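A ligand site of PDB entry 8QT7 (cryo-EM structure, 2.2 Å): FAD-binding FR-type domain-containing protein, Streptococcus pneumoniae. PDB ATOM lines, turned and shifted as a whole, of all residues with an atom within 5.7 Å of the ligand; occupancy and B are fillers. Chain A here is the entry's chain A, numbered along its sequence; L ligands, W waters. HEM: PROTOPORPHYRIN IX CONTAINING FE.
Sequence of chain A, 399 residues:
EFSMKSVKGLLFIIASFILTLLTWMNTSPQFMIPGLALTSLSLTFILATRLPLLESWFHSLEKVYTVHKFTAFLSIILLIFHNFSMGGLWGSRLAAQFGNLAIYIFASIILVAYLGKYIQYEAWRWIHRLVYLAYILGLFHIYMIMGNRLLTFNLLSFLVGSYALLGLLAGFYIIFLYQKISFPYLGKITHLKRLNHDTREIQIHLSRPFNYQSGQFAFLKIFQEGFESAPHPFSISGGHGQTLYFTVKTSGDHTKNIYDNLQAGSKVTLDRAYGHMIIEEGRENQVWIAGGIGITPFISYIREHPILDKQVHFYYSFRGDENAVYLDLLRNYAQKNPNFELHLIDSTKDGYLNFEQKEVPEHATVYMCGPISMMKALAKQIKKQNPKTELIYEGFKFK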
ATOM      1  N   TRP A  24      -4.411  -5.744 -12.937  1.00  0.00           N
ATOM      2  CA  TRP A  24      -4.002  -4.367 -12.723  1.00  0.00           C
ATOM      3  C   TRP A  24      -4.054  -3.998 -11.243  1.00  0.00           C
ATOM      4  O   TRP A  24      -3.118  -3.396 -10.717  1.00  0.00           O
ATOM      5  CB  TRP A  24      -4.894  -3.426 -13.534  1.00  0.00           C
ATOM      6  CG  TRP A  24      -4.571  -3.434 -14.994  1.00  0.00           C
ATOM      7  CD1 TRP A  24      -5.234  -4.098 -15.979  1.00  0.00           C
ATOM      8  CD2 TRP A  24      -3.479  -2.756 -15.624  1.00  0.00           C
ATOM      9  NE1 TRP A  24      -4.632  -3.871 -17.188  1.00  0.00           N
ATOM     10  CE2 TRP A  24      -3.551  -3.045 -17.004  1.00  0.00           C
ATOM     11  CE3 TRP A  24      -2.450  -1.930 -15.167  1.00  0.00           C
ATOM     12  CZ2 TRP A  24      -2.642  -2.542 -17.919  1.00  0.00           C
ATOM     13  CZ3 TRP A  24      -1.547  -1.419 -16.077  1.00  0.00           C
ATOM     14  CH2 TRP A  24      -1.652  -1.732 -17.441  1.00  0.00           C
ATOM     15  N   PHE A  31      -4.198   2.147 -13.056  1.00  0.00           N
ATOM     16  CA  PHE A  31      -4.530   1.933 -14.463  1.00  0.00           C
ATOM     17  C   PHE A  31      -5.599   0.866 -14.664  1.00  0.00           C
ATOM     18  O   PHE A  31      -5.653   0.251 -15.728  1.00  0.00           O
ATOM     19  CB  PHE A  31      -3.267   1.559 -15.252  1.00  0.00           C
ATOM     20  CG  PHE A  31      -2.187   2.600 -15.190  1.00  0.00           C
ATOM     21  CD1 PHE A  31      -2.449   3.922 -15.514  1.00  0.00           C
ATOM     22  CD2 PHE A  31      -0.899   2.244 -14.812  1.00  0.00           C
ATOM     23  CE1 PHE A  31      -1.441   4.869 -15.450  1.00  0.00           C
ATOM     24  CE2 PHE A  31       0.109   3.197 -14.757  1.00  0.00           C
ATOM     25  CZ  PHE A  31      -0.169   4.504 -15.080  1.00  0.00           C
ATOM     26  N   PRO A  34      -8.138   2.345 -17.612  1.00  0.00           N
ATOM     27  CA  PRO A  34      -7.677   2.212 -18.996  1.00  0.00           C
ATOM     28  C   PRO A  34      -7.342   0.779 -19.381  1.00  0.00           C
ATOM     29  O   PRO A  34      -7.698   0.340 -20.483  1.00  0.00           O
ATOM     30  CB  PRO A  34      -6.451   3.134 -19.058  1.00  0.00           C
ATOM     31  CG  PRO A  34      -5.976   3.208 -17.669  1.00  0.00           C
ATOM     32  CD  PRO A  34      -7.186   3.148 -16.804  1.00  0.00           C
ATOM     33  N   GLY A  35      -6.685   0.034 -18.489  1.00  0.00           N
ATOM     34  CA  GLY A  35      -6.327  -1.342 -18.810  1.00  0.00           C
ATOM     35  C   GLY A  35      -7.553  -2.183 -19.141  1.00  0.00           C
ATOM     36  O   GLY A  35      -7.585  -2.882 -20.151  1.00  0.00           O
ATOM     37  N   ALA A  37     -10.304  -1.017 -20.252  1.00  0.00           N
ATOM     38  CA  ALA A  37     -10.720  -0.532 -21.560  1.00  0.00           C
ATOM     39  C   ALA A  37      -9.985  -1.278 -22.672  1.00  0.00           C
ATOM     40  O   ALA A  37     -10.604  -1.744 -23.627  1.00  0.00           O
ATOM     41  CB  ALA A  37     -10.474   0.977 -21.676  1.00  0.00           C
ATOM     42  N   LEU A  38      -8.668  -1.454 -22.509  1.00  0.00           N
ATOM     43  CA  LEU A  38      -7.893  -2.164 -23.520  1.00  0.00           C
ATOM     44  C   LEU A  38      -8.495  -3.540 -23.779  1.00  0.00           C
ATOM     45  O   LEU A  38      -8.733  -3.917 -24.934  1.00  0.00           O
ATOM     46  CB  LEU A  38      -6.435  -2.294 -23.067  1.00  0.00           C
ATOM     47  CG  LEU A  38      -5.506  -2.981 -24.057  1.00  0.00           C
ATOM     48  CD1 LEU A  38      -5.416  -2.195 -25.358  1.00  0.00           C
ATOM     49  CD2 LEU A  38      -4.123  -3.178 -23.452  1.00  0.00           C
ATOM     50  N   LEU A  41     -11.516  -3.309 -25.759  1.00  0.00           N
ATOM     51  CA  LEU A  41     -11.186  -3.042 -27.154  1.00  0.00           C
ATOM     52  C   LEU A  41     -10.857  -4.349 -27.868  1.00  0.00           C
ATOM     53  O   LEU A  41     -11.426  -4.638 -28.927  1.00  0.00           O
ATOM     54  CB  LEU A  41     -10.015  -2.065 -27.246  1.00  0.00           C
ATOM     55  CG  LEU A  41     -10.305  -0.584 -27.029  1.00  0.00           C
ATOM     56  CD1 LEU A  41      -9.018   0.225 -27.003  1.00  0.00           C
ATOM     57  CD2 LEU A  41     -11.253  -0.053 -28.098  1.00  0.00           C
ATOM     58  N   LEU A  79     -12.607   4.884 -21.687  1.00  0.00           N
ATOM     59  CA  LEU A  79     -11.568   5.735 -22.243  1.00  0.00           C
ATOM     60  C   LEU A  79     -11.852   7.210 -21.981  1.00  0.00           C
ATOM     61  O   LEU A  79     -10.930   7.986 -21.728  1.00  0.00           O
ATOM     62  CB  LEU A  79     -11.420   5.474 -23.737  1.00  0.00           C
ATOM     63  CG  LEU A  79     -10.691   4.179 -24.082  1.00  0.00           C
ATOM     64  CD1 LEU A  79     -10.590   3.983 -25.585  1.00  0.00           C
ATOM     65  CD2 LEU A  79      -9.328   4.137 -23.422  1.00  0.00           C
ATOM     66  N   HIS A  82     -10.904   7.791 -18.413  1.00  0.00           N
ATOM     67  CA  HIS A  82      -9.447   7.820 -18.314  1.00  0.00           C
ATOM     68  C   HIS A  82      -8.884   9.144 -18.809  1.00  0.00           C
ATOM     69  O   HIS A  82      -7.994   9.732 -18.178  1.00  0.00           O
ATOM     70  CB  HIS A  82      -8.877   6.631 -19.114  1.00  0.00           C
ATOM     71  CG  HIS A  82      -7.402   6.716 -19.362  1.00  0.00           C
ATOM     72  ND1 HIS A  82      -6.475   6.737 -18.346  1.00  0.00           N
ATOM     73  CD2 HIS A  82      -6.704   6.735 -20.519  1.00  0.00           C
ATOM     74  CE1 HIS A  82      -5.254   6.782 -18.868  1.00  0.00           C
ATOM     75  NE2 HIS A  82      -5.367   6.787 -20.188  1.00  0.00           N
ATOM     76  N   ASN A  83      -9.392   9.640 -19.950  1.00  0.00           N
ATOM     77  CA  ASN A  83      -8.943  10.924 -20.474  1.00  0.00           C
ATOM     78  C   ASN A  83      -9.271  12.065 -19.521  1.00  0.00           C
ATOM     79  O   ASN A  83      -8.451  12.962 -19.307  1.00  0.00           O
ATOM     80  CB  ASN A  83      -9.582  11.174 -21.844  1.00  0.00           C
ATOM     81  CG  ASN A  83      -8.976  12.354 -22.578  1.00  0.00           C
ATOM     82  OD1 ASN A  83      -8.079  13.026 -22.083  1.00  0.00           O
ATOM     83  ND2 ASN A  83      -9.466  12.600 -23.789  1.00  0.00           N
ATOM     84  N   MET A  86      -6.873  11.785 -16.420  1.00  0.00           N
ATOM     85  CA  MET A  86      -5.430  11.800 -16.647  1.00  0.00           C
ATOM     86  C   MET A  86      -4.913  13.052 -17.342  1.00  0.00           C
ATOM     87  O   MET A  86      -3.875  13.572 -16.945  1.00  0.00           O
ATOM     88  CB  MET A  86      -5.009  10.576 -17.463  1.00  0.00           C
ATOM     89  CG  MET A  86      -5.032   9.287 -16.676  1.00  0.00           C
ATOM     90  SD  MET A  86      -3.558   9.052 -15.662  1.00  0.00           S
ATOM     91  CE  MET A  86      -4.174   7.869 -14.458  1.00  0.00           C
ATOM     92  N   GLY A  87      -5.609  13.545 -18.361  1.00  0.00           N
ATOM     93  CA  GLY A  87      -5.114  14.707 -19.083  1.00  0.00           C
ATOM     94  C   GLY A  87      -6.196  15.678 -19.531  1.00  0.00           C
ATOM     95  O   GLY A  87      -7.138  15.954 -18.784  1.00  0.00           O
ATOM     96  N   GLY A  88      -6.049  16.198 -20.738  1.00  0.00           N
ATOM     97  CA  GLY A  88      -6.999  17.141 -21.288  1.00  0.00           C
ATOM     98  C   GLY A  88      -7.348  16.865 -22.738  1.00  0.00           C
ATOM     99  O   GLY A  88      -7.717  15.737 -23.094  1.00  0.00           O
ATOM    100  N   LEU A  89      -7.218  17.878 -23.590  1.00  0.00           N
ATOM    101  CA  LEU A  89      -7.593  17.759 -24.999  1.00  0.00           C
ATOM    102  C   LEU A  89      -6.403  17.505 -25.909  1.00  0.00           C
ATOM    103  O   LEU A  89      -6.599  16.941 -27.003  1.00  0.00           O
ATOM    104  CB  LEU A  89      -8.321  19.024 -25.462  1.00  0.00           C
ATOM    105  CG  LEU A  89      -9.708  19.246 -24.851  1.00  0.00           C
ATOM    106  CD1 LEU A  89     -10.106  20.711 -24.899  1.00  0.00           C
ATOM    107  CD2 LEU A  89     -10.741  18.381 -25.552  1.00  0.00           C
ATOM    108  N   TRP A  90      -5.199  17.894 -25.509  1.00  0.00           N
ATOM    109  CA  TRP A  90      -4.002  17.641 -26.309  1.00  0.00           C
ATOM    110  C   TRP A  90      -2.805  17.600 -25.376  1.00  0.00           C
ATOM    111  O   TRP A  90      -2.601  18.521 -24.585  1.00  0.00           O
ATOM    112  CB  TRP A  90      -3.811  18.718 -27.378  1.00  0.00           C
ATOM    113  CG  TRP A  90      -2.848  18.334 -28.462  1.00  0.00           C
ATOM    114  CD1 TRP A  90      -1.669  18.944 -28.765  1.00  0.00           C
ATOM    115  CD2 TRP A  90      -2.984  17.248 -29.393  1.00  0.00           C
ATOM    116  NE1 TRP A  90      -1.054  18.306 -29.818  1.00  0.00           N
ATOM    117  CE2 TRP A  90      -1.846  17.261 -30.214  1.00  0.00           C
ATOM    118  CE3 TRP A  90      -3.947  16.263 -29.599  1.00  0.00           C
ATOM    119  CZ2 TRP A  90      -1.649  16.333 -31.232  1.00  0.00           C
ATOM    120  CZ3 TRP A  90      -3.757  15.336 -30.605  1.00  0.00           C
ATOM    121  CH2 TRP A  90      -2.620  15.384 -31.413  1.00  0.00           C
ATOM    122  N   GLY A  91      -2.022  16.523 -25.459  1.00  0.00           N
ATOM    123  CA  GLY A  91      -0.903  16.348 -24.565  1.00  0.00           C
ATOM    124  C   GLY A  91       0.325  17.124 -24.980  1.00  0.00           C
ATOM    125  O   GLY A  91       0.398  17.728 -26.043  1.00  0.00           O
ATOM    126  N   SER A  92       1.324  17.097 -24.098  1.00  0.00           N
ATOM    127  CA  SER A  92       2.580  17.789 -24.348  1.00  0.00           C
ATOM    128  C   SER A  92       3.621  16.873 -24.995  1.00  0.00           C
ATOM    129  O   SER A  92       4.414  17.326 -25.824  1.00  0.00           O
ATOM    130  CB  SER A  92       3.142  18.368 -23.044  1.00  0.00           C
ATOM    131  OG  SER A  92       3.155  17.405 -22.008  1.00  0.00           O
ATOM    132  N   ARG A  93       3.626  15.603 -24.629  1.00  0.00           N
ATOM    133  CA  ARG A  93       4.535  14.622 -25.214  1.00  0.00           C
ATOM    134  C   ARG A  93       3.812  13.808 -26.283  1.00  0.00           C
ATOM    135  O   ARG A  93       2.584  13.738 -26.311  1.00  0.00           O
ATOM    136  CB  ARG A  93       5.106  13.706 -24.132  1.00  0.00           C
ATOM    137  CG  ARG A  93       4.054  12.924 -23.361  1.00  0.00           C
ATOM    138  CD  ARG A  93       4.556  12.532 -21.981  1.00  0.00           C
ATOM    139  NE  ARG A  93       5.540  11.458 -22.038  1.00  0.00           N
ATOM    140  CZ  ARG A  93       5.499  10.365 -21.291  1.00  0.00           C
ATOM    141  NH1 ARG A  93       4.530  10.162 -20.410  1.00  0.00           N
ATOM    142  NH2 ARG A  93       6.451   9.453 -21.424  1.00  0.00           N
ATOM    143  N   ALA A  96       1.354  10.980 -25.115  1.00  0.00           N
ATOM    144  CA  ALA A  96       0.021  11.441 -24.735  1.00  0.00           C
ATOM    145  C   ALA A  96      -0.795  11.839 -25.954  1.00  0.00           C
ATOM    146  O   ALA A  96      -2.013  11.603 -26.008  1.00  0.00           O
ATOM    147  CB  ALA A  96       0.129  12.619 -23.757  1.00  0.00           C
ATOM    148  N   GLN A  97      -0.151  12.436 -26.956  1.00  0.00           N
ATOM    149  CA  GLN A  97      -0.858  12.851 -28.162  1.00  0.00           C
ATOM    150  C   GLN A  97      -1.344  11.642 -28.962  1.00  0.00           C
ATOM    151  O   GLN A  97      -2.370  11.729 -29.637  1.00  0.00           O
ATOM    152  CB  GLN A  97       0.039  13.737 -29.025  1.00  0.00           C
ATOM    153  CG  GLN A  97       0.346  15.072 -28.391  1.00  0.00           C
ATOM    154  CD  GLN A  97       1.633  15.680 -28.901  1.00  0.00           C
ATOM    155  OE1 GLN A  97       2.276  15.133 -29.792  1.00  0.00           O
ATOM    156  NE2 GLN A  97       2.017  16.820 -28.341  1.00  0.00           N
ATOM    157  N   GLY A  99      -2.556   8.913 -27.562  1.00  0.00           N
ATOM    158  CA  GLY A  99      -3.817   8.613 -26.913  1.00  0.00           C
ATOM    159  C   GLY A  99      -4.905   9.603 -27.251  1.00  0.00           C
ATOM    160  O   GLY A  99      -6.065   9.228 -27.430  1.00  0.00           O
ATOM    161  N   ASN A 100      -4.551  10.891 -27.323  1.00  0.00           N
ATOM    162  CA  ASN A 100      -5.526  11.910 -27.714  1.00  0.00           C
ATOM    163  C   ASN A 100      -6.101  11.612 -29.096  1.00  0.00           C
ATOM    164  O   ASN A 100      -7.326  11.598 -29.293  1.00  0.00           O
ATOM    165  CB  ASN A 100      -4.878  13.293 -27.700  1.00  0.00           C
ATOM    166  CG  ASN A 100      -4.854  13.917 -26.317  1.00  0.00           C
ATOM    167  OD1 ASN A 100      -3.800  14.308 -25.824  1.00  0.00           O
ATOM    168  ND2 ASN A 100      -6.017  14.010 -25.694  1.00  0.00           N
ATOM    169  N   ALA A 102      -6.083   8.745 -30.718  1.00  0.00           N
ATOM    170  CA  ALA A 102      -6.819   7.487 -30.706  1.00  0.00           C
ATOM    171  C   ALA A 102      -8.211   7.669 -30.135  1.00  0.00           C
ATOM    172  O   ALA A 102      -9.187   7.131 -30.682  1.00  0.00           O
ATOM    173  CB  ALA A 102      -6.037   6.441 -29.907  1.00  0.00           C
ATOM    174  N   ILE A 103      -8.348   8.437 -29.049  1.00  0.00           N
ATOM    175  CA  ILE A 103      -9.660   8.629 -28.449  1.00  0.00           C
ATOM    176  C   ILE A 103     -10.545   9.474 -29.360  1.00  0.00           C
ATOM    177  O   ILE A 103     -11.756   9.231 -29.467  1.00  0.00           O
ATOM    178  CB  ILE A 103      -9.547   9.222 -27.028  1.00  0.00           C
ATOM    179  CG1 ILE A 103     -10.786   8.845 -26.211  1.00  0.00           C
ATOM    180  CG2 ILE A 103      -9.380  10.739 -27.051  1.00  0.00           C
ATOM    181  CD1 ILE A 103     -10.726   9.289 -24.764  1.00  0.00           C
ATOM    182  N   PHE A 106     -11.732   7.097 -32.048  1.00  0.00           N
ATOM    183  CA  PHE A 106     -12.700   6.153 -31.498  1.00  0.00           C
ATOM    184  C   PHE A 106     -14.066   6.809 -31.306  1.00  0.00           C
ATOM    185  O   PHE A 106     -15.098   6.242 -31.685  1.00  0.00           O
ATOM    186  CB  PHE A 106     -12.195   5.602 -30.165  1.00  0.00           C
ATOM    187  CG  PHE A 106     -11.310   4.396 -30.298  1.00  0.00           C
ATOM    188  CD1 PHE A 106     -11.647   3.356 -31.137  1.00  0.00           C
ATOM    189  CD2 PHE A 106     -10.126   4.308 -29.581  1.00  0.00           C
ATOM    190  CE1 PHE A 106     -10.834   2.244 -31.263  1.00  0.00           C
ATOM    191  CE2 PHE A 106      -9.311   3.207 -29.700  1.00  0.00           C
ATOM    192  CZ  PHE A 106      -9.661   2.174 -30.547  1.00  0.00           C
ATOM    193  N   ALA A 134      -6.983   3.721 -34.993  1.00  0.00           N
ATOM    194  CA  ALA A 134      -7.136   4.215 -33.634  1.00  0.00           C
ATOM    195  C   ALA A 134      -6.545   3.237 -32.616  1.00  0.00           C
ATOM    196  O   ALA A 134      -5.893   3.645 -31.660  1.00  0.00           O
ATOM    197  CB  ALA A 134      -8.617   4.459 -33.333  1.00  0.00           C
ATOM    198  N   GLY A 138      -3.466   3.713 -30.030  1.00  0.00           N
ATOM    199  CA  GLY A 138      -3.585   3.431 -28.609  1.00  0.00           C
ATOM    200  C   GLY A 138      -2.523   2.470 -28.108  1.00  0.00           C
ATOM    201  O   GLY A 138      -2.004   2.626 -26.998  1.00  0.00           O
ATOM    202  N   HIS A 141       0.585   4.399 -27.749  1.00  0.00           N
ATOM    203  CA  HIS A 141       0.480   5.234 -26.554  1.00  0.00           C
ATOM    204  C   HIS A 141       0.795   4.425 -25.295  1.00  0.00           C
ATOM    205  O   HIS A 141       1.607   4.841 -24.461  1.00  0.00           O
ATOM    206  CB  HIS A 141      -0.938   5.826 -26.507  1.00  0.00           C
ATOM    207  CG  HIS A 141      -1.413   6.225 -25.152  1.00  0.00           C
ATOM    208  ND1 HIS A 141      -1.238   7.497 -24.636  1.00  0.00           N
ATOM    209  CD2 HIS A 141      -2.114   5.543 -24.213  1.00  0.00           C
ATOM    210  CE1 HIS A 141      -1.792   7.572 -23.447  1.00  0.00           C
ATOM    211  NE2 HIS A 141      -2.318   6.385 -23.157  1.00  0.00           N
ATOM    212  N   ILE A 142       0.193   3.242 -25.181  1.00  0.00           N
ATOM    213  CA  ILE A 142       0.401   2.390 -24.012  1.00  0.00           C
ATOM    214  C   ILE A 142       1.856   1.952 -23.913  1.00  0.00           C
ATOM    215  O   ILE A 142       2.464   1.988 -22.837  1.00  0.00           O
ATOM    216  CB  ILE A 142      -0.542   1.170 -24.058  1.00  0.00           C
ATOM    217  CG1 ILE A 142      -1.996   1.623 -23.977  1.00  0.00           C
ATOM    218  CG2 ILE A 142      -0.228   0.214 -22.924  1.00  0.00           C
ATOM    219  CD1 ILE A 142      -2.969   0.605 -24.521  1.00  0.00           C
ATOM    220  N   ILE A 145       4.213   4.996 -22.958  1.00  0.00           N
ATOM    221  CA  ILE A 145       4.086   5.434 -21.560  1.00  0.00           C
ATOM    222  C   ILE A 145       4.619   4.358 -20.615  1.00  0.00           C
ATOM    223  O   ILE A 145       5.361   4.652 -19.677  1.00  0.00           O
ATOM    224  CB  ILE A 145       2.645   5.841 -21.230  1.00  0.00           C
ATOM    225  CG1 ILE A 145       2.449   7.305 -21.620  1.00  0.00           C
ATOM    226  CG2 ILE A 145       2.336   5.625 -19.762  1.00  0.00           C
ATOM    227  CD1 ILE A 145       1.084   7.618 -22.072  1.00  0.00           C
ATOM    228  N   MET A 146       4.243   3.099 -20.854  1.00  0.00           N
ATOM    229  CA  MET A 146       4.792   1.977 -20.108  1.00  0.00           C
ATOM    230  C   MET A 146       5.901   1.351 -20.951  1.00  0.00           C
ATOM    231  O   MET A 146       5.635   0.839 -22.043  1.00  0.00           O
ATOM    232  CB  MET A 146       3.712   0.954 -19.770  1.00  0.00           C
ATOM    233  CG  MET A 146       2.379   1.550 -19.373  1.00  0.00           C
ATOM    234  SD  MET A 146       2.216   1.777 -17.588  1.00  0.00           S
ATOM    235  CE  MET A 146       1.857   0.105 -17.062  1.00  0.00           C
HETATM  236  CHA HEM L   1      -3.235   9.838 -20.805  1.00  0.00           C
HETATM  237  CHB HEM L   1      -1.559   5.591 -19.341  1.00  0.00           C
HETATM  238  CHC HEM L   1      -4.718   3.456 -22.331  1.00  0.00           C
HETATM  239  CHD HEM L   1      -6.000   7.736 -24.080  1.00  0.00           C
HETATM  240  C1A HEM L   1      -2.502   8.884 -20.167  1.00  0.00           C
HETATM  241  C2A HEM L   1      -1.521   9.112 -19.198  1.00  0.00           C
HETATM  242  C3A HEM L   1      -1.072   7.930 -18.782  1.00  0.00           C
HETATM  243  C4A HEM L   1      -1.739   6.938 -19.481  1.00  0.00           C
HETATM  244  CMA HEM L   1      -0.018   7.762 -17.746  1.00  0.00           C
HETATM  245  CAA HEM L   1      -1.045  10.424 -18.645  1.00  0.00           C
HETATM  246  CBA HEM L   1      -0.624  11.418 -19.720  1.00  0.00           C
HETATM  247  CGA HEM L   1       0.859  11.603 -19.802  1.00  0.00           C
HETATM  248  O1A HEM L   1       1.624  10.639 -19.956  1.00  0.00           O
HETATM  249  O2A HEM L   1       1.312  12.754 -19.761  1.00  0.00           O
HETATM  250  C1B HEM L   1      -2.328   4.633 -20.003  1.00  0.00           C
HETATM  251  C2B HEM L   1      -2.210   3.255 -19.781  1.00  0.00           C
HETATM  252  C3B HEM L   1      -3.107   2.665 -20.621  1.00  0.00           C
HETATM  253  C4B HEM L   1      -3.766   3.717 -21.367  1.00  0.00           C
HETATM  254  CMB HEM L   1      -1.278   2.579 -18.812  1.00  0.00           C
HETATM  255  CAB HEM L   1      -3.413   1.261 -20.830  1.00  0.00           C
HETATM  256  CBB HEM L   1      -3.641   0.446 -19.843  1.00  0.00           C
HETATM  257  C1C HEM L   1      -5.259   4.394 -23.176  1.00  0.00           C
HETATM  258  C2C HEM L   1      -5.950   4.181 -24.356  1.00  0.00           C
HETATM  259  C3C HEM L   1      -6.315   5.436 -24.846  1.00  0.00           C
HETATM  260  C4C HEM L   1      -5.820   6.388 -23.940  1.00  0.00           C
HETATM  261  CMC HEM L   1      -6.220   2.807 -24.916  1.00  0.00           C
HETATM  262  CAC HEM L   1      -7.069   5.871 -26.032  1.00  0.00           C
HETATM  263  CBC HEM L   1      -7.530   5.082 -26.993  1.00  0.00           C
HETATM  264  C1D HEM L   1      -5.361   8.646 -23.282  1.00  0.00           C
HETATM  265  C2D HEM L   1      -5.586  10.071 -23.423  1.00  0.00           C
HETATM  266  C3D HEM L   1      -4.827  10.660 -22.515  1.00  0.00           C
HETATM  267  C4D HEM L   1      -4.134   9.591 -21.814  1.00  0.00           C
HETATM  268  CMD HEM L   1      -6.500  10.727 -24.405  1.00  0.00           C
HETATM  269  CAD HEM L   1      -4.689  12.133 -22.255  1.00  0.00           C
HETATM  270  CBD HEM L   1      -3.446  12.681 -22.932  1.00  0.00           C
HETATM  271  CGD HEM L   1      -3.125  14.012 -22.371  1.00  0.00           C
HETATM  272  O1D HEM L   1      -2.067  14.210 -21.814  1.00  0.00           O
HETATM  273  O2D HEM L   1      -3.865  14.993 -22.434  1.00  0.00           O
HETATM  274  NA  HEM L   1      -2.590   7.545 -20.330  1.00  0.00           N
HETATM  275  NB  HEM L   1      -3.247   4.851 -20.941  1.00  0.00           N
HETATM  276  NC  HEM L   1      -5.172   5.722 -22.947  1.00  0.00           N
HETATM  277  ND  HEM L   1      -4.480   8.416 -22.307  1.00  0.00           N
HETATM  278 FE   HEM L   1      -3.846   6.742 -21.659  1.00  0.00          FE
HETATM  279  O   HOH W   1      -3.499  17.828 -22.112  1.00  0.00           O
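The guanidinium group (NH1) of Arg 93 is in salt-bridge range of an oxygen (O1A) of the ligand (3.0 Å).
The backbone NH (N) of Gly 88 lies within hydrogen-bond range of an oxygen (O2D) of the ligand (3.0 Å).
A ring nitrogen (NE2) of His 82 is bound to an iron atom (FE) of the ligand.
NE2 of His 141 binds FE of the ligand, at 2.2 Å.
An oxygen (O2D) of the ligand lies close to the side-chain amide oxygen (OD1) of Asn 100 (3.5 Å).
OD1 of Asn 100 sits close to O of Ala 96.
N of Gly 91 is in hydrogen-bond range of OD1 of Asn 100 (2.9 Å).
The backbone carbonyl oxygen (O) of Gly 91 is in hydrogen-bond range of the side-chain amide nitrogen (NE2) of Gln 97 (3.0 Å).
The side-chain amide nitrogen (ND2) of Asn 100 is in hydrogen-bond range of the backbone carbonyl oxygen (O) of Leu 89, at 3.3 Å.
The side-chain amide oxygen of Asn 83 sits close to the backbone carbonyl oxygen of Gly 88.
Merely in contact with the ligand: Ala 96 (3.3 Å), Gly 35 (3.4 Å), Gly 99 (3.4 Å), Ile 142 (3.5 Å), Asn 83 (3.5 Å), Leu 79 (3.5 Å), Ala 102 (3.5 Å), Gly 87 (3.6 Å), Pro 34 (3.6 Å), Gly 91 (3.7 Å), Trp 24 (3.7 Å), Ile 145 (3.7 Å), Phe 31 (3.7 Å), Phe 106 (3.7 Å), Met 146 (3.8 Å), Met 86 (3.9 Å) and Ile 103 (3.9 Å).
22 residues have an atom within 4 Å of the ligand: Trp 24, Phe 31, Pro 34, Gly 35, Leu 79, His 82, Asn 83, Met 86, Gly 87, Gly 88, Gly 91, Arg 93, Ala 96, Gly 99, Asn 100, Ala 102, Ile 103, Phe 106, His 141, Ile 142, Ile 145 and Met 146.
The nearest printed residue that does not touch the ligand is Trp 90 (4.1 Å).
Water W1 lies within hydrogen-bond range of the backbone carbonyl oxygen (O) of Trp 90, an oxygen (O2D) of the ligand and the backbone NH (N) of Gly 88.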
